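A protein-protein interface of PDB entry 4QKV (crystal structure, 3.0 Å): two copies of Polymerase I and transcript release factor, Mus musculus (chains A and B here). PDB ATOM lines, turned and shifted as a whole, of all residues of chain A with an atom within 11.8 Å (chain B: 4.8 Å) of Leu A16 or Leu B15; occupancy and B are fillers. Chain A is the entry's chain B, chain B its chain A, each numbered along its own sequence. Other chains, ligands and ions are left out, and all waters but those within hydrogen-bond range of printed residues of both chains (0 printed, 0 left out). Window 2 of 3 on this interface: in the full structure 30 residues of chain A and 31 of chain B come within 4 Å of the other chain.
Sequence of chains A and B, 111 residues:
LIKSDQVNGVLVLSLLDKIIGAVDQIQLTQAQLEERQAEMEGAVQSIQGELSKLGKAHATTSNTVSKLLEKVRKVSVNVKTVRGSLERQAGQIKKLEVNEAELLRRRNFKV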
ATOM      1  N   ASN A   8      -7.481  -0.271   7.665  1.00  0.00           N
ATOM      2  CA  ASN A   8      -7.064   0.365   6.425  1.00  0.00           C
ATOM      3  C   ASN A   8      -5.664  -0.081   6.009  1.00  0.00           C
ATOM      4  O   ASN A   8      -5.284   0.024   4.833  1.00  0.00           O
ATOM      5  CB  ASN A   8      -7.129   1.899   6.548  1.00  0.00           C
ATOM      6  CG  ASN A   8      -5.822   2.534   7.049  1.00  0.00           C
ATOM      7  OD1 ASN A   8      -4.975   1.886   7.672  1.00  0.00           O
ATOM      8  ND2 ASN A   8      -5.652   3.819   6.746  1.00  0.00           N
ATOM      9  N   GLY A   9      -4.890  -0.542   6.992  1.00  0.00           N
ATOM     10  CA  GLY A   9      -3.568  -1.086   6.735  1.00  0.00           C
ATOM     11  C   GLY A   9      -3.673  -2.290   5.815  1.00  0.00           C
ATOM     12  O   GLY A   9      -2.777  -2.563   5.019  1.00  0.00           O
ATOM     13  N   VAL A  10      -4.785  -3.013   5.940  1.00  0.00           N
ATOM     14  CA  VAL A  10      -5.108  -4.126   5.053  1.00  0.00           C
ATOM     15  C   VAL A  10      -5.323  -3.612   3.617  1.00  0.00           C
ATOM     16  O   VAL A  10      -4.883  -4.238   2.659  1.00  0.00           O
ATOM     17  CB  VAL A  10      -6.370  -4.911   5.567  1.00  0.00           C
ATOM     18  CG1 VAL A  10      -7.416  -5.122   4.453  1.00  0.00           C
ATOM     19  CG2 VAL A  10      -5.958  -6.246   6.176  1.00  0.00           C
ATOM     20  N   LEU A  11      -5.965  -2.454   3.492  1.00  0.00           N
ATOM     21  CA  LEU A  11      -6.247  -1.853   2.197  1.00  0.00           C
ATOM     22  C   LEU A  11      -4.958  -1.389   1.525  1.00  0.00           C
ATOM     23  O   LEU A  11      -4.842  -1.413   0.295  1.00  0.00           O
ATOM     24  CB  LEU A  11      -7.226  -0.674   2.341  1.00  0.00           C
ATOM     25  CG  LEU A  11      -8.668  -0.989   2.773  1.00  0.00           C
ATOM     26  CD1 LEU A  11      -9.660   0.025   2.226  1.00  0.00           C
ATOM     27  CD2 LEU A  11      -9.077  -2.402   2.358  1.00  0.00           C
ATOM     28  N   VAL A  12      -3.994  -0.966   2.341  1.00  0.00           N
ATOM     29  CA  VAL A  12      -2.703  -0.521   1.832  1.00  0.00           C
ATOM     30  C   VAL A  12      -1.906  -1.686   1.266  1.00  0.00           C
ATOM     31  O   VAL A  12      -1.380  -1.594   0.160  1.00  0.00           O
ATOM     32  CB  VAL A  12      -1.881   0.188   2.922  1.00  0.00           C
ATOM     33  CG1 VAL A  12      -0.406   0.189   2.568  1.00  0.00           C
ATOM     34  CG2 VAL A  12      -2.382   1.608   3.110  1.00  0.00           C
ATOM     35  N   LEU A  13      -1.827  -2.782   2.012  1.00  0.00           N
ATOM     36  CA  LEU A  13      -1.148  -3.988   1.537  1.00  0.00           C
ATOM     37  C   LEU A  13      -1.890  -4.615   0.336  1.00  0.00           C
ATOM     38  O   LEU A  13      -1.265  -5.105  -0.624  1.00  0.00           O
ATOM     39  CB  LEU A  13      -1.010  -5.002   2.677  1.00  0.00           C
ATOM     40  CG  LEU A  13       0.231  -4.899   3.572  1.00  0.00           C
ATOM     41  CD1 LEU A  13       0.418  -3.494   4.091  1.00  0.00           C
ATOM     42  CD2 LEU A  13       0.133  -5.876   4.732  1.00  0.00           C
ATOM     43  N   SER A  14      -3.221  -4.567   0.408  1.00  0.00           N
ATOM     44  CA  SER A  14      -4.104  -5.028  -0.654  1.00  0.00           C
ATOM     45  C   SER A  14      -3.824  -4.302  -1.963  1.00  0.00           C
ATOM     46  O   SER A  14      -3.948  -4.871  -3.058  1.00  0.00           O
ATOM     47  CB  SER A  14      -5.556  -4.822  -0.233  1.00  0.00           C
ATOM     48  OG  SER A  14      -6.444  -4.867  -1.324  1.00  0.00           O
ATOM     49  N   LEU A  15      -3.438  -3.039  -1.823  1.00  0.00           N
ATOM     50  CA  LEU A  15      -3.143  -2.164  -2.946  1.00  0.00           C
ATOM     51  C   LEU A  15      -1.681  -2.292  -3.329  1.00  0.00           C
ATOM     52  O   LEU A  15      -1.270  -1.925  -4.435  1.00  0.00           O
ATOM     53  CB  LEU A  15      -3.464  -0.724  -2.574  1.00  0.00           C
ATOM     54  CG  LEU A  15      -3.415   0.354  -3.644  1.00  0.00           C
ATOM     55  CD1 LEU A  15      -4.381  -0.001  -4.767  1.00  0.00           C
ATOM     56  CD2 LEU A  15      -3.734   1.731  -3.031  1.00  0.00           C
ATOM     57  N   LEU A  16      -0.884  -2.824  -2.413  1.00  0.00           N
ATOM     58  CA  LEU A  16       0.535  -2.911  -2.673  1.00  0.00           C
ATOM     59  C   LEU A  16       0.860  -4.118  -3.521  1.00  0.00           C
ATOM     60  O   LEU A  16       1.666  -4.031  -4.438  1.00  0.00           O
ATOM     61  CB  LEU A  16       1.331  -2.972  -1.381  1.00  0.00           C
ATOM     62  CG  LEU A  16       2.648  -2.216  -1.562  1.00  0.00           C
ATOM     63  CD1 LEU A  16       2.317  -0.799  -1.963  1.00  0.00           C
ATOM     64  CD2 LEU A  16       3.497  -2.212  -0.313  1.00  0.00           C
ATOM     65  N   ASP A  17       0.241  -5.251  -3.222  1.00  0.00           N
ATOM     66  CA  ASP A  17       0.511  -6.434  -4.021  1.00  0.00           C
ATOM     67  C   ASP A  17      -0.231  -6.375  -5.364  1.00  0.00           C
ATOM     68  O   ASP A  17       0.102  -7.114  -6.296  1.00  0.00           O
ATOM     69  CB  ASP A  17       0.154  -7.702  -3.246  1.00  0.00           C
ATOM     70  CG  ASP A  17      -1.331  -7.925  -3.147  1.00  0.00           C
ATOM     71  OD1 ASP A  17      -2.096  -6.933  -3.146  1.00  0.00           O
ATOM     72  OD2 ASP A  17      -1.728  -9.106  -3.066  1.00  0.00           O
ATOM     73  N   LYS A  18      -1.224  -5.492  -5.471  1.00  0.00           N
ATOM     74  CA  LYS A  18      -1.826  -5.220  -6.772  1.00  0.00           C
ATOM     75  C   LYS A  18      -0.852  -4.425  -7.637  1.00  0.00           C
ATOM     76  O   LYS A  18      -0.673  -4.715  -8.820  1.00  0.00           O
ATOM     77  CB  LYS A  18      -3.158  -4.475  -6.644  1.00  0.00           C
ATOM     78  CG  LYS A  18      -4.335  -5.391  -6.352  1.00  0.00           C
ATOM     79  CD  LYS A  18      -5.657  -4.768  -6.786  1.00  0.00           C
ATOM     80  CE  LYS A  18      -6.758  -5.826  -6.858  1.00  0.00           C
ATOM     81  NZ  LYS A  18      -8.086  -5.261  -7.247  1.00  0.00           N
ATOM     82  N   ILE A  19      -0.225  -3.418  -7.043  1.00  0.00           N
ATOM     83  CA  ILE A  19       0.821  -2.677  -7.734  1.00  0.00           C
ATOM     84  C   ILE A  19       1.975  -3.598  -8.089  1.00  0.00           C
ATOM     85  O   ILE A  19       2.528  -3.513  -9.170  1.00  0.00           O
ATOM     86  CB  ILE A  19       1.341  -1.511  -6.881  1.00  0.00           C
ATOM     87  CG1 ILE A  19       0.291  -0.400  -6.822  1.00  0.00           C
ATOM     88  CG2 ILE A  19       2.674  -0.992  -7.419  1.00  0.00           C
ATOM     89  CD1 ILE A  19       0.771   0.822  -6.089  1.00  0.00           C
ATOM     90  N   ILE A  20       2.339  -4.479  -7.169  1.00  0.00           N
ATOM     91  CA  ILE A  20       3.405  -5.419  -7.439  1.00  0.00           C
ATOM     92  C   ILE A  20       3.068  -6.264  -8.664  1.00  0.00           C
ATOM     93  O   ILE A  20       3.896  -6.423  -9.559  1.00  0.00           O
ATOM     94  CB  ILE A  20       3.670  -6.338  -6.256  1.00  0.00           C
ATOM     95  CG1 ILE A  20       4.373  -5.576  -5.140  1.00  0.00           C
ATOM     96  CG2 ILE A  20       4.550  -7.479  -6.681  1.00  0.00           C
ATOM     97  CD1 ILE A  20       4.660  -6.440  -3.939  1.00  0.00           C
ATOM     98  N   GLY A  21       1.840  -6.776  -8.708  1.00  0.00           N
ATOM     99  CA  GLY A  21       1.408  -7.640  -9.791  1.00  0.00           C
ATOM    100  C   GLY A  21       1.541  -6.996 -11.155  1.00  0.00           C
ATOM    101  O   GLY A  21       1.982  -7.633 -12.129  1.00  0.00           O
ATOM    102  N   ALA A  22       1.149  -5.726 -11.209  1.00  0.00           N
ATOM    103  CA  ALA A  22       1.193  -4.906 -12.409  1.00  0.00           C
ATOM    104  C   ALA A  22       2.608  -4.804 -12.935  1.00  0.00           C
ATOM    105  O   ALA A  22       2.884  -5.145 -14.089  1.00  0.00           O
ATOM    106  CB  ALA A  22       0.642  -3.521 -12.114  1.00  0.00           C
ATOM    107  N   VAL A  23       3.498  -4.336 -12.070  1.00  0.00           N
ATOM    108  CA  VAL A  23       4.904  -4.182 -12.406  1.00  0.00           C
ATOM    109  C   VAL A  23       5.532  -5.531 -12.807  1.00  0.00           C
ATOM    110  O   VAL A  23       6.422  -5.588 -13.667  1.00  0.00           O
ATOM    111  CB  VAL A  23       5.671  -3.551 -11.223  1.00  0.00           C
ATOM    112  CG1 VAL A  23       7.141  -3.384 -11.558  1.00  0.00           C
ATOM    113  CG2 VAL A  23       5.073  -2.214 -10.900  1.00  0.00           C
ATOM    114  N   ASP A  24       5.057  -6.616 -12.202  1.00  0.00           N
ATOM    115  CA  ASP A  24       5.521  -7.936 -12.586  1.00  0.00           C
ATOM    116  C   ASP A  24       5.241  -8.155 -14.051  1.00  0.00           C
ATOM    117  O   ASP A  24       6.139  -8.528 -14.810  1.00  0.00           O
ATOM    118  CB  ASP A  24       4.860  -9.021 -11.751  1.00  0.00           C
ATOM    119  CG  ASP A  24       5.485  -9.141 -10.385  1.00  0.00           C
ATOM    120  OD1 ASP A  24       6.583  -8.569 -10.203  1.00  0.00           O
ATOM    121  OD2 ASP A  24       4.890  -9.795  -9.496  1.00  0.00           O
ATOM    122  N   GLN A  25       3.998  -7.895 -14.443  1.00  0.00           N
ATOM    123  CA  GLN A  25       3.566  -8.162 -15.804  1.00  0.00           C
ATOM    124  C   GLN A  25       4.253  -7.216 -16.779  1.00  0.00           C
ATOM    125  O   GLN A  25       4.718  -7.641 -17.843  1.00  0.00           O
ATOM    126  CB  GLN A  25       2.044  -8.047 -15.914  1.00  0.00           C
ATOM    127  CG  GLN A  25       1.456  -8.578 -17.225  1.00  0.00           C
ATOM    128  CD  GLN A  25       1.721 -10.063 -17.466  1.00  0.00           C
ATOM    129  OE1 GLN A  25       1.909 -10.849 -16.526  1.00  0.00           O
ATOM    130  NE2 GLN A  25       1.721 -10.452 -18.738  1.00  0.00           N
ATOM    131  N   GLN A  27       7.130  -5.779 -16.460  1.00  0.00           N
ATOM    132  CA  GLN A  27       8.490  -6.255 -16.667  1.00  0.00           C
ATOM    133  C   GLN A  27       8.520  -7.426 -17.669  1.00  0.00           C
ATOM    134  O   GLN A  27       9.402  -7.492 -18.516  1.00  0.00           O
ATOM    135  CB  GLN A  27       9.142  -6.663 -15.331  1.00  0.00           C
ATOM    136  CG  GLN A  27       9.545  -5.461 -14.477  1.00  0.00           C
ATOM    137  CD  GLN A  27      10.347  -5.809 -13.213  1.00  0.00           C
ATOM    138  OE1 GLN A  27      10.052  -6.789 -12.512  1.00  0.00           O
ATOM    139  NE2 GLN A  27      11.358  -4.983 -12.911  1.00  0.00           N
ATOM    140  N   LEU B  11       7.963  -4.061   6.333  1.00  0.00           N
ATOM    141  CA  LEU B  11       7.430  -4.688   5.115  1.00  0.00           C
ATOM    142  C   LEU B  11       7.149  -3.651   4.033  1.00  0.00           C
ATOM    143  O   LEU B  11       7.785  -3.668   2.984  1.00  0.00           O
ATOM    144  CB  LEU B  11       6.144  -5.462   5.418  1.00  0.00           C
ATOM    145  CG  LEU B  11       6.214  -6.971   5.643  1.00  0.00           C
ATOM    146  CD1 LEU B  11       7.300  -7.305   6.644  1.00  0.00           C
ATOM    147  CD2 LEU B  11       4.865  -7.487   6.147  1.00  0.00           C
ATOM    148  N   VAL B  12       6.201  -2.755   4.310  1.00  0.00           N
ATOM    149  CA  VAL B  12       5.841  -1.682   3.391  1.00  0.00           C
ATOM    150  C   VAL B  12       7.077  -0.953   2.883  1.00  0.00           C
ATOM    151  O   VAL B  12       7.234  -0.766   1.674  1.00  0.00           O
ATOM    152  CB  VAL B  12       4.873  -0.665   4.050  1.00  0.00           C
ATOM    153  CG1 VAL B  12       4.824   0.642   3.276  1.00  0.00           C
ATOM    154  CG2 VAL B  12       3.485  -1.251   4.153  1.00  0.00           C
ATOM    155  N   LEU B  13       7.966  -0.568   3.793  1.00  0.00           N
ATOM    156  CA  LEU B  13       9.164   0.160   3.384  1.00  0.00           C
ATOM    157  C   LEU B  13      10.010  -0.600   2.360  1.00  0.00           C
ATOM    158  O   LEU B  13      10.346  -0.043   1.315  1.00  0.00           O
ATOM    159  CB  LEU B  13      10.007   0.534   4.603  1.00  0.00           C
ATOM    160  CG  LEU B  13       9.515   1.847   5.217  1.00  0.00           C
ATOM    161  CD1 LEU B  13      10.511   2.422   6.231  1.00  0.00           C
ATOM    162  CD2 LEU B  13       9.228   2.855   4.107  1.00  0.00           C
ATOM    163  N   SER B  14      10.324  -1.865   2.628  1.00  0.00           N
ATOM    164  CA  SER B  14      11.180  -2.638   1.718  1.00  0.00           C
ATOM    165  C   SER B  14      10.493  -2.960   0.383  1.00  0.00           C
ATOM    166  O   SER B  14      11.131  -2.924  -0.666  1.00  0.00           O
ATOM    167  CB  SER B  14      11.651  -3.927   2.397  1.00  0.00           C
ATOM    168  OG  SER B  14      10.575  -4.817   2.617  1.00  0.00           O
ATOM    169  N   LEU B  15       9.199  -3.275   0.426  1.00  0.00           N
ATOM    170  CA  LEU B  15       8.395  -3.406  -0.784  1.00  0.00           C
ATOM    171  C   LEU B  15       8.389  -2.105  -1.579  1.00  0.00           C
ATOM    172  O   LEU B  15       8.820  -2.075  -2.727  1.00  0.00           O
ATOM    173  CB  LEU B  15       6.957  -3.804  -0.452  1.00  0.00           C
ATOM    174  CG  LEU B  15       6.714  -5.188   0.166  1.00  0.00           C
ATOM    175  CD1 LEU B  15       5.217  -5.438   0.309  1.00  0.00           C
ATOM    176  CD2 LEU B  15       7.386  -6.324  -0.618  1.00  0.00           C
ATOM    177  N   LEU B  16       7.895  -1.033  -0.966  1.00  0.00           N
ATOM    178  CA  LEU B  16       7.872   0.271  -1.626  1.00  0.00           C
ATOM    179  C   LEU B  16       9.187   0.602  -2.306  1.00  0.00           C
ATOM    180  O   LEU B  16       9.207   1.067  -3.447  1.00  0.00           O
ATOM    181  CB  LEU B  16       7.525   1.383  -0.634  1.00  0.00           C
ATOM    182  CG  LEU B  16       6.023   1.632  -0.490  1.00  0.00           C
ATOM    183  CD1 LEU B  16       5.778   2.962   0.149  1.00  0.00           C
ATOM    184  CD2 LEU B  16       5.332   1.574  -1.843  1.00  0.00           C
ATOM    185  N   ASP B  17      10.288   0.333  -1.621  1.00  0.00           N
ATOM    186  CA  ASP B  17      11.584   0.698  -2.162  1.00  0.00           C
ATOM    187  C   ASP B  17      11.972  -0.140  -3.389  1.00  0.00           C
ATOM    188  O   ASP B  17      12.615   0.368  -4.309  1.00  0.00           O
ATOM    189  CB  ASP B  17      12.662   0.582  -1.086  1.00  0.00           C
ATOM    190  CG  ASP B  17      13.678   1.705  -1.172  1.00  0.00           C
ATOM    191  OD1 ASP B  17      13.286   2.851  -1.502  1.00  0.00           O
ATOM    192  OD2 ASP B  17      14.871   1.437  -0.932  1.00  0.00           O
ATOM    193  N   LYS B  18      11.585  -1.414  -3.399  1.00  0.00           N
ATOM    194  CA  LYS B  18      11.933  -2.300  -4.517  1.00  0.00           C
ATOM    195  C   LYS B  18      11.009  -2.071  -5.719  1.00  0.00           C
ATOM    196  O   LYS B  18      11.462  -2.110  -6.861  1.00  0.00           O
ATOM    197  CB  LYS B  18      11.934  -3.772  -4.071  1.00  0.00           C
ATOM    198  CG  LYS B  18      13.197  -4.094  -3.245  1.00  0.00           C
ATOM    199  CD  LYS B  18      13.216  -5.460  -2.552  1.00  0.00           C
ATOM    200  CE  LYS B  18      12.849  -6.607  -3.476  1.00  0.00           C
ATOM    201  NZ  LYS B  18      13.194  -7.941  -2.881  1.00  0.00           N
ATOM    202  N   ILE B  19       9.737  -1.786  -5.451  1.00  0.00           N
ATOM    203  CA  ILE B  19       8.802  -1.297  -6.459  1.00  0.00           C
ATOM    204  C   ILE B  19       9.352  -0.082  -7.205  1.00  0.00           C
ATOM    205  O   ILE B  19       9.297  -0.028  -8.435  1.00  0.00           O
ATOM    206  CB  ILE B  19       7.440  -0.923  -5.819  1.00  0.00           C
ATOM    207  CG1 ILE B  19       6.668  -2.185  -5.424  1.00  0.00           C
ATOM    208  CG2 ILE B  19       6.606  -0.086  -6.758  1.00  0.00           C
ATOM    209  CD1 ILE B  19       5.300  -1.912  -4.840  1.00  0.00           C
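Among the printed residues, pairs that only touch across the chains: Leu A13 with Val B12, Leu A16 with Leu B15, Leu A16 with Leu B16, Ile A19 with Ile B19 and Ile A20 with Ile B19.
Of the printed residues of chain B, Leu A16 touches Leu B15 and Leu B16.
Of chain A, only Leu A16 (3.7 Å) comes within 4 Å of Leu B15.
No residue of chain A comes within 4 Å of Leu B11.
No residue of chain A comes within 4 Å of Asp B17.
No residue of chain A comes within 4 Å of Lys B18.
Of chain A, only Ile A19 (3.8 Å) and Ile A20 (3.8 Å) come within 4 Å of Ile B19.
Of the printed residues of chain B, Leu A13 touches Val B12.
Printed residues of chain B within 4 Å of Ile A19: Ile B19.
Of the printed residues of chain B, Ile A20 touches Ile B19 (3.8 Å).
Asp A24 touches none of the printed residues of chain B.
The nearest residue of chain B that does not touch Leu A16 is Ile B19 (4.2 Å).
The nearest printed residue of chain B that does not touch Leu A13 is Leu B11 (5.2 Å).
Hydrophobic or aromatic side chains of chain B within 4 Å of the printed part of chain A: Val B12, Leu B15, Leu B16 and Ile B19.
Among the printed residues, 5 pairs touch across the chains.
Among the printed residues, no Asp or Glu carboxylate lies within 4 Å of a Lys or Arg side-chain nitrogen of the other chain.
Leu A13 touches Val B12, but with the chains exchanged Val A12 does not touch Leu B13 (8.5 Å).
Leu A16 touches Leu B15, but with the chains exchanged Leu A15 does not touch Leu B16 (7.9 Å).
Leu B16 touches its own counterpart, Leu A16.
Ile A19 touches its own counterpart, Ile B19.
Positions printed for both chains: 11, 12, 13, 14, 15, 16, 17, 18 and 19.
Of the 5 pairs that touch across the chains among the printed residues, 2 have their exchanged pair printed and touching as well.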
